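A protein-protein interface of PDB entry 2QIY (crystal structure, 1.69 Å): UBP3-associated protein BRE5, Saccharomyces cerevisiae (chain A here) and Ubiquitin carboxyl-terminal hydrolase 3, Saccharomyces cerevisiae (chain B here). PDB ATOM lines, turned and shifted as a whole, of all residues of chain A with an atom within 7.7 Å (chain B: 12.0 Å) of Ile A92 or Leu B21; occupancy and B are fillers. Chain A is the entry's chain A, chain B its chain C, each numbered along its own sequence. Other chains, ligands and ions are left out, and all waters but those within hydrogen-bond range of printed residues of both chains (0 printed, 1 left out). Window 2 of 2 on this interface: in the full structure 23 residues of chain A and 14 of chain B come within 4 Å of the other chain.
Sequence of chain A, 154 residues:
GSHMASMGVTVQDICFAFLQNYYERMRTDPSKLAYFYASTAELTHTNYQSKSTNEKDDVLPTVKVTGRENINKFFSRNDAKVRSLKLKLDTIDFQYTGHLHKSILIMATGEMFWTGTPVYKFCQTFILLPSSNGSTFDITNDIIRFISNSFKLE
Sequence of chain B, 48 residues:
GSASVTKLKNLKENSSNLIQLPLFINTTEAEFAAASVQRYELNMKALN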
ATOM      1  N   VAL A  11     -12.550  33.300 -24.034  1.00  0.00           N
ATOM      2  CA  VAL A  11     -13.700  32.716 -24.723  1.00  0.00           C
ATOM      3  C   VAL A  11     -14.373  31.635 -23.862  1.00  0.00           C
ATOM      4  O   VAL A  11     -15.604  31.554 -23.816  1.00  0.00           O
ATOM      5  CB  VAL A  11     -13.343  32.225 -26.158  1.00  0.00           C
ATOM      6  CG1 VAL A  11     -12.196  31.222 -26.136  1.00  0.00           C
ATOM      7  CG2 VAL A  11     -14.571  31.661 -26.863  1.00  0.00           C
ATOM      8  N   GLN A  12     -13.577  30.829 -23.159  1.00  0.00           N
ATOM      9  CA  GLN A  12     -14.145  29.838 -22.239  1.00  0.00           C
ATOM     10  C   GLN A  12     -14.968  30.527 -21.145  1.00  0.00           C
ATOM     11  O   GLN A  12     -16.068  30.080 -20.803  1.00  0.00           O
ATOM     12  CB  GLN A  12     -13.059  28.962 -21.609  1.00  0.00           C
ATOM     13  CG  GLN A  12     -13.634  27.807 -20.796  1.00  0.00           C
ATOM     14  CD  GLN A  12     -12.594  27.080 -19.976  1.00  0.00           C
ATOM     15  OE1 GLN A  12     -12.012  27.640 -19.037  1.00  0.00           O
ATOM     16  NE2 GLN A  12     -12.354  25.821 -20.321  1.00  0.00           N
ATOM     17  N   CYS A  15     -18.305  31.768 -22.571  1.00  0.00           N
ATOM     18  CA  CYS A  15     -19.219  30.630 -22.807  1.00  0.00           C
ATOM     19  C   CYS A  15     -19.828  30.115 -21.513  1.00  0.00           C
ATOM     20  O   CYS A  15     -21.018  29.830 -21.456  1.00  0.00           O
ATOM     21  CB  CYS A  15     -18.517  29.483 -23.518  1.00  0.00           C
ATOM     22  SG  CYS A  15     -18.066  29.879 -25.190  1.00  0.00           S
ATOM     23  N   PHE A  16     -19.008  30.012 -20.468  1.00  0.00           N
ATOM     24  CA  PHE A  16     -19.497  29.510 -19.199  1.00  0.00           C
ATOM     25  C   PHE A  16     -20.497  30.491 -18.587  1.00  0.00           C
ATOM     26  O   PHE A  16     -21.581  30.073 -18.143  1.00  0.00           O
ATOM     27  CB  PHE A  16     -18.343  29.210 -18.246  1.00  0.00           C
ATOM     28  CG  PHE A  16     -18.774  28.536 -16.981  1.00  0.00           C
ATOM     29  CD1 PHE A  16     -18.848  27.148 -16.910  1.00  0.00           C
ATOM     30  CD2 PHE A  16     -19.101  29.293 -15.850  1.00  0.00           C
ATOM     31  CE1 PHE A  16     -19.243  26.514 -15.728  1.00  0.00           C
ATOM     32  CE2 PHE A  16     -19.497  28.674 -14.662  1.00  0.00           C
ATOM     33  CZ  PHE A  16     -19.569  27.279 -14.599  1.00  0.00           C
ATOM     34  N   ALA A  17     -20.157  31.783 -18.615  1.00  0.00           N
ATOM     35  CA  ALA A  17     -21.051  32.845 -18.135  1.00  0.00           C
ATOM     36  C   ALA A  17     -22.333  32.898 -18.952  1.00  0.00           C
ATOM     37  O   ALA A  17     -23.426  33.029 -18.386  1.00  0.00           O
ATOM     38  CB  ALA A  17     -20.353  34.210 -18.144  1.00  0.00           C
ATOM     39  N   LEU A  19     -23.900  30.496 -20.572  1.00  0.00           N
ATOM     40  CA  LEU A  19     -24.797  29.372 -20.313  1.00  0.00           C
ATOM     41  C   LEU A  19     -25.422  29.525 -18.942  1.00  0.00           C
ATOM     42  O   LEU A  19     -26.626  29.328 -18.773  1.00  0.00           O
ATOM     43  CB  LEU A  19     -24.021  28.065 -20.371  1.00  0.00           C
ATOM     44  CG  LEU A  19     -23.981  27.106 -21.568  1.00  0.00           C
ATOM     45  CD1 LEU A  19     -24.807  27.465 -22.812  1.00  0.00           C
ATOM     46  CD2 LEU A  19     -22.593  26.601 -21.854  1.00  0.00           C
ATOM     47  N   GLN A  20     -24.604  29.882 -17.952  1.00  0.00           N
ATOM     48  CA  GLN A  20     -25.140  30.027 -16.597  1.00  0.00           C
ATOM     49  C   GLN A  20     -26.214  31.114 -16.566  1.00  0.00           C
ATOM     50  O   GLN A  20     -27.301  30.891 -16.035  1.00  0.00           O
ATOM     51  CB  GLN A  20     -24.031  30.250 -15.557  1.00  0.00           C
ATOM     52  CG  GLN A  20     -24.481  29.766 -14.175  1.00  0.00           C
ATOM     53  CD  GLN A  20     -23.361  29.681 -13.141  1.00  0.00           C
ATOM     54  OE1 GLN A  20     -22.181  29.852 -13.450  1.00  0.00           O
ATOM     55  NE2 GLN A  20     -23.742  29.409 -11.895  1.00  0.00           N
ATOM     56  N   LYS A  88     -28.606  19.526 -14.978  1.00  0.00           N
ATOM     57  CA  LYS A  88     -27.211  19.200 -14.723  1.00  0.00           C
ATOM     58  C   LYS A  88     -26.476  19.467 -16.027  1.00  0.00           C
ATOM     59  O   LYS A  88     -26.772  18.842 -17.054  1.00  0.00           O
ATOM     60  CB  LYS A  88     -27.083  17.739 -14.313  1.00  0.00           C
ATOM     61  CG  LYS A  88     -25.647  17.296 -14.126  1.00  0.00           C
ATOM     62  CD  LYS A  88     -25.556  15.865 -13.611  1.00  0.00           C
ATOM     63  CE  LYS A  88     -24.098  15.481 -13.433  1.00  0.00           C
ATOM     64  NZ  LYS A  88     -23.957  14.132 -12.819  1.00  0.00           N
ATOM     65  N   LEU A  89     -25.594  20.461 -16.018  1.00  0.00           N
ATOM     66  CA  LEU A  89     -24.807  20.813 -17.225  1.00  0.00           C
ATOM     67  C   LEU A  89     -23.529  19.970 -17.184  1.00  0.00           C
ATOM     68  O   LEU A  89     -22.725  20.114 -16.260  1.00  0.00           O
ATOM     69  CB  LEU A  89     -24.449  22.312 -17.203  1.00  0.00           C
ATOM     70  CG  LEU A  89     -24.191  23.179 -18.446  1.00  0.00           C
ATOM     71  CD1 LEU A  89     -23.038  24.151 -18.238  1.00  0.00           C
ATOM     72  CD2 LEU A  89     -24.193  22.476 -19.839  1.00  0.00           C
ATOM     73  N   ASP A  90     -23.347  19.079 -18.167  1.00  0.00           N
ATOM     74  CA  ASP A  90     -22.214  18.135 -18.159  1.00  0.00           C
ATOM     75  C   ASP A  90     -20.985  18.618 -18.949  1.00  0.00           C
ATOM     76  O   ASP A  90     -19.840  18.424 -18.522  1.00  0.00           O
ATOM     77  CB  ASP A  90     -22.616  16.789 -18.763  1.00  0.00           C
ATOM     78  CG  ASP A  90     -23.541  15.966 -17.866  1.00  0.00           C
ATOM     79  OD1 ASP A  90     -24.409  15.296 -18.443  1.00  0.00           O
ATOM     80  OD2 ASP A  90     -23.390  15.948 -16.622  1.00  0.00           O
ATOM     81  N   THR A  91     -21.231  19.165 -20.133  1.00  0.00           N
ATOM     82  CA  THR A  91     -20.155  19.482 -21.069  1.00  0.00           C
ATOM     83  C   THR A  91     -20.394  20.787 -21.808  1.00  0.00           C
ATOM     84  O   THR A  91     -21.541  21.191 -22.056  1.00  0.00           O
ATOM     85  CB  THR A  91     -19.958  18.366 -22.148  1.00  0.00           C
ATOM     86  OG1 THR A  91     -21.075  18.358 -23.039  1.00  0.00           O
ATOM     87  CG2 THR A  91     -19.859  16.981 -21.502  1.00  0.00           C
ATOM     88  N   ILE A  92     -19.284  21.438 -22.167  1.00  0.00           N
ATOM     89  CA  ILE A  92     -19.334  22.623 -22.994  1.00  0.00           C
ATOM     90  C   ILE A  92     -18.237  22.462 -24.046  1.00  0.00           C
ATOM     91  O   ILE A  92     -17.092  22.096 -23.698  1.00  0.00           O
ATOM     92  CB  ILE A  92     -19.028  23.908 -22.179  1.00  0.00           C
ATOM     93  CG1 ILE A  92     -20.044  24.079 -21.024  1.00  0.00           C
ATOM     94  CG2 ILE A  92     -18.969  25.144 -23.108  1.00  0.00           C
ATOM     95  CD1 ILE A  92     -19.698  25.168 -20.004  1.00  0.00           C
ATOM     96  N   ASP A  93     -18.600  22.745 -25.303  1.00  0.00           N
ATOM     97  CA  ASP A  93     -17.643  22.834 -26.428  1.00  0.00           C
ATOM     98  C   ASP A  93     -17.869  24.161 -27.120  1.00  0.00           C
ATOM     99  O   ASP A  93     -19.001  24.608 -27.242  1.00  0.00           O
ATOM    100  CB  ASP A  93     -17.897  21.724 -27.453  1.00  0.00           C
ATOM    101  CG  ASP A  93     -17.654  20.351 -26.888  1.00  0.00           C
ATOM    102  OD1 ASP A  93     -16.470  19.986 -26.749  1.00  0.00           O
ATOM    103  OD2 ASP A  93     -18.641  19.646 -26.574  1.00  0.00           O
ATOM    104  N   PHE A  94     -16.791  24.798 -27.585  1.00  0.00           N
ATOM    105  CA  PHE A  94     -16.976  26.024 -28.364  1.00  0.00           C
ATOM    106  C   PHE A  94     -15.985  26.141 -29.496  1.00  0.00           C
ATOM    107  O   PHE A  94     -14.896  25.545 -29.456  1.00  0.00           O
ATOM    108  CB  PHE A  94     -16.889  27.266 -27.472  1.00  0.00           C
ATOM    109  CG  PHE A  94     -15.573  27.393 -26.746  1.00  0.00           C
ATOM    110  CD1 PHE A  94     -14.491  28.016 -27.352  1.00  0.00           C
ATOM    111  CD2 PHE A  94     -15.421  26.867 -25.464  1.00  0.00           C
ATOM    112  CE1 PHE A  94     -13.271  28.131 -26.684  1.00  0.00           C
ATOM    113  CE2 PHE A  94     -14.188  26.972 -24.786  1.00  0.00           C
ATOM    114  CZ  PHE A  94     -13.126  27.597 -25.397  1.00  0.00           C
ATOM    115  N   LEU A 105     -19.734  29.715 -31.530  1.00  0.00           N
ATOM    116  CA  LEU A 105     -20.544  28.488 -31.553  1.00  0.00           C
ATOM    117  C   LEU A 105     -20.348  27.773 -30.237  1.00  0.00           C
ATOM    118  O   LEU A 105     -19.209  27.481 -29.865  1.00  0.00           O
ATOM    119  CB  LEU A 105     -20.014  27.566 -32.665  1.00  0.00           C
ATOM    120  CG  LEU A 105     -20.842  26.475 -33.380  1.00  0.00           C
ATOM    121  CD1 LEU A 105     -20.034  25.260 -33.895  1.00  0.00           C
ATOM    122  CD2 LEU A 105     -22.227  26.113 -32.805  1.00  0.00           C
ATOM    123  N   ILE A 106     -21.449  27.494 -29.525  1.00  0.00           N
ATOM    124  CA  ILE A 106     -21.389  26.799 -28.254  1.00  0.00           C
ATOM    125  C   ILE A 106     -22.245  25.526 -28.310  1.00  0.00           C
ATOM    126  O   ILE A 106     -23.377  25.559 -28.772  1.00  0.00           O
ATOM    127  CB  ILE A 106     -21.888  27.699 -27.075  1.00  0.00           C
ATOM    128  CG1 ILE A 106     -21.102  29.007 -27.020  1.00  0.00           C
ATOM    129  CG2 ILE A 106     -21.801  26.945 -25.745  1.00  0.00           C
ATOM    130  CD1 ILE A 106     -21.648  30.031 -25.972  1.00  0.00           C
ATOM    131  N   MET A 107     -21.714  24.409 -27.834  1.00  0.00           N
ATOM    132  CA  MET A 107     -22.587  23.239 -27.636  1.00  0.00           C
ATOM    133  C   MET A 107     -22.538  22.812 -26.187  1.00  0.00           C
ATOM    134  O   MET A 107     -21.445  22.698 -25.613  1.00  0.00           O
ATOM    135  CB  MET A 107     -22.114  22.041 -28.439  1.00  0.00           C
ATOM    136  CG  MET A 107     -22.222  22.123 -29.897  1.00  0.00           C
ATOM    137  SD  MET A 107     -21.502  20.562 -30.467  1.00  0.00           S
ATOM    138  CE  MET A 107     -22.801  19.445 -30.047  1.00  0.00           C
ATOM    139  N   ALA A 108     -23.708  22.555 -25.601  1.00  0.00           N
ATOM    140  CA  ALA A 108     -23.790  22.114 -24.215  1.00  0.00           C
ATOM    141  C   ALA A 108     -24.507  20.775 -24.179  1.00  0.00           C
ATOM    142  O   ALA A 108     -25.377  20.510 -25.018  1.00  0.00           O
ATOM    143  CB  ALA A 108     -24.554  23.125 -23.418  1.00  0.00           C
ATOM    144  N   THR A 109     -24.155  19.903 -23.243  1.00  0.00           N
ATOM    145  CA  THR A 109     -24.974  18.689 -23.097  1.00  0.00           C
ATOM    146  C   THR A 109     -25.187  18.484 -21.629  1.00  0.00           C
ATOM    147  O   THR A 109     -24.383  18.947 -20.801  1.00  0.00           O
ATOM    148  CB  THR A 109     -24.331  17.380 -23.664  1.00  0.00           C
ATOM    149  OG1 THR A 109     -23.311  16.890 -22.769  1.00  0.00           O
ATOM    150  CG2 THR A 109     -23.735  17.587 -25.053  1.00  0.00           C
ATOM    151  N   LEU B  21     -17.321  21.688 -13.932  1.00  0.00           N
ATOM    152  CA  LEU B  21     -18.446  20.839 -14.465  1.00  0.00           C
ATOM    153  C   LEU B  21     -18.396  19.451 -13.834  1.00  0.00           C
ATOM    154  O   LEU B  21     -17.300  18.956 -13.536  1.00  0.00           O
ATOM    155  CB  LEU B  21     -18.363  20.707 -15.990  1.00  0.00           C
ATOM    156  CG  LEU B  21     -18.540  21.950 -16.866  1.00  0.00           C
ATOM    157  CD1 LEU B  21     -18.418  21.567 -18.340  1.00  0.00           C
ATOM    158  CD2 LEU B  21     -19.871  22.625 -16.627  1.00  0.00           C
ATOM    159  N   PRO B  22     -19.565  18.815 -13.622  1.00  0.00           N
ATOM    160  CA  PRO B  22     -20.928  19.311 -13.943  1.00  0.00           C
ATOM    161  C   PRO B  22     -21.411  20.417 -13.009  1.00  0.00           C
ATOM    162  O   PRO B  22     -20.992  20.487 -11.834  1.00  0.00           O
ATOM    163  CB  PRO B  22     -21.806  18.073 -13.755  1.00  0.00           C
ATOM    164  CG  PRO B  22     -21.074  17.282 -12.714  1.00  0.00           C
ATOM    165  CD  PRO B  22     -19.615  17.465 -13.033  1.00  0.00           C
ATOM    166  N   LEU B  23     -22.269  21.273 -13.548  1.00  0.00           N
ATOM    167  CA  LEU B  23     -22.859  22.385 -12.824  1.00  0.00           C
ATOM    168  C   LEU B  23     -24.346  22.092 -12.678  1.00  0.00           C
ATOM    169  O   LEU B  23     -25.021  21.790 -13.660  1.00  0.00           O
ATOM    170  CB  LEU B  23     -22.710  23.667 -13.654  1.00  0.00           C
ATOM    171  CG  LEU B  23     -22.287  25.034 -13.124  1.00  0.00           C
ATOM    172  CD1 LEU B  23     -22.953  26.132 -13.950  1.00  0.00           C
ATOM    173  CD2 LEU B  23     -22.506  25.265 -11.618  1.00  0.00           C
ATOM    174  N   PHE B  24     -24.853  22.160 -11.453  1.00  0.00           N
ATOM    175  CA  PHE B  24     -26.301  22.093 -11.240  1.00  0.00           C
ATOM    176  C   PHE B  24     -26.842  23.504 -11.328  1.00  0.00           C
ATOM    177  O   PHE B  24     -26.322  24.425 -10.663  1.00  0.00           O
ATOM    178  CB  PHE B  24     -26.602  21.415  -9.896  1.00  0.00           C
ATOM    179  CG  PHE B  24     -26.117  20.007  -9.862  1.00  0.00           C
ATOM    180  CD1 PHE B  24     -24.818  19.711  -9.449  1.00  0.00           C
ATOM    181  CD2 PHE B  24     -26.916  18.992 -10.376  1.00  0.00           C
ATOM    182  CE1 PHE B  24     -24.343  18.411  -9.500  1.00  0.00           C
ATOM    183  CE2 PHE B  24     -26.452  17.683 -10.429  1.00  0.00           C
ATOM    184  CZ  PHE B  24     -25.176  17.393  -9.979  1.00  0.00           C
ATOM    185  N   ILE B  25     -27.841  23.690 -12.188  1.00  0.00           N
ATOM    186  CA  ILE B  25     -28.364  25.029 -12.500  1.00  0.00           C
ATOM    187  C   ILE B  25     -29.848  25.059 -12.161  1.00  0.00           C
ATOM    188  O   ILE B  25     -30.608  24.202 -12.605  1.00  0.00           O
ATOM    189  CB  ILE B  25     -28.109  25.413 -13.972  1.00  0.00           C
ATOM    190  CG1 ILE B  25     -26.610  25.299 -14.306  1.00  0.00           C
ATOM    191  CG2 ILE B  25     -28.587  26.855 -14.270  1.00  0.00           C
ATOM    192  CD1 ILE B  25     -26.256  25.693 -15.705  1.00  0.00           C
ATOM    193  N   GLU B  29     -27.866  18.954  -6.368  1.00  0.00           N
ATOM    194  CA  GLU B  29     -27.525  17.586  -6.698  1.00  0.00           C
ATOM    195  C   GLU B  29     -28.607  16.611  -6.220  1.00  0.00           C
ATOM    196  O   GLU B  29     -28.938  15.656  -6.932  1.00  0.00           O
ATOM    197  CB  GLU B  29     -26.169  17.218  -6.093  1.00  0.00           C
ATOM    198  CG  GLU B  29     -25.704  15.860  -6.558  1.00  0.00           C
ATOM    199  CD  GLU B  29     -24.225  15.630  -6.360  1.00  0.00           C
ATOM    200  OE1 GLU B  29     -23.541  16.482  -5.739  1.00  0.00           O
ATOM    201  OE2 GLU B  29     -23.746  14.579  -6.845  1.00  0.00           O
ATOM    202  N   PHE B  32     -31.727  16.797  -8.467  1.00  0.00           N
ATOM    203  CA  PHE B  32     -31.337  16.110  -9.690  1.00  0.00           C
ATOM    204  C   PHE B  32     -31.364  14.582  -9.515  1.00  0.00           C
ATOM    205  O   PHE B  32     -31.920  13.852 -10.347  1.00  0.00           O
ATOM    206  CB  PHE B  32     -29.952  16.530 -10.201  1.00  0.00           C
ATOM    207  CG  PHE B  32     -29.468  15.626 -11.290  1.00  0.00           C
ATOM    208  CD1 PHE B  32     -29.976  15.768 -12.580  1.00  0.00           C
ATOM    209  CD2 PHE B  32     -28.588  14.572 -11.012  1.00  0.00           C
ATOM    210  CE1 PHE B  32     -29.576  14.890 -13.593  1.00  0.00           C
ATOM    211  CE2 PHE B  32     -28.188  13.680 -12.052  1.00  0.00           C
ATOM    212  CZ  PHE B  32     -28.691  13.857 -13.311  1.00  0.00           C
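The backbone carbonyl oxygen (O) of Leu B23 lies within hydrogen-bond range of the backbone NH (N) of Leu A89 (2.8 Å).
The side-chain hydroxyl of Thr A91 is in hydrogen-bond range of the side-chain hydroxyl of Thr A109.
The backbone NH of Asp A90 sits at hydrogen-bond distance from the backbone carbonyl oxygen of Thr A109 (2.8 Å).
CZ of Phe A16 touches CD1 of Leu B23, at 3.6 Å.
Gln A20 touches Leu B23 (CD to CD1, 3.7 Å).
Pro B22 touches Lys A88.
CD of Lys A88 touches CE2 of Phe B24, at 3.8 Å.
Lys A88 touches Phe B32.
Leu B21 touches Leu A89 (CD2 to O, 3.8 Å).
Leu A89 touches Pro B22.
Pro B22 touches Asp A90.
Thr A91 touches Leu B21 (CA to CD1, 3.8 Å).
Leu B21 touches Ile A92 (CD1 to N, 3.9 Å).
Val A11 touches none of the printed residues of chain B.
No residue of chain B comes within 4 Å of Cys A15.
Of the printed residues of chain B, Gln A20 touches Leu B23 (3.7 Å).
Printed residues of chain B within 4 Å of Lys A88: Pro B22, Leu B23, Phe B24 and Phe B32.
Leu A89 touches just these residues of chain B: Leu B21, Pro B22 and Leu B23.
Of chain B, only Leu B21 comes within 4 Å of Thr A91.
Ile A92 touches just one residue of chain B: Leu B21.
No residue of chain B comes within 4 Å of Asp A93.
Ile A106 touches none of the printed residues of chain B.
Leu B21 touches just these residues of chain A: Leu A89 (3.8 Å), Asp A90 (3.5 Å), Thr A91 (3.8 Å) and Ile A92 (3.9 Å).
Of the printed residues of chain A, Leu B23 touches Phe A16 (3.6 Å), Gln A20 (3.7 Å), Lys A88 (3.6 Å) and Leu A89 (2.8 Å).
Of the printed residues of chain A, Phe B24 touches Lys A88.
The nearest residue of chain B that does not touch Ile A92 is Leu B23 (6.9 Å).
Of the 19 printed residues of chain A, 7 touch a printed residue of chain B.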
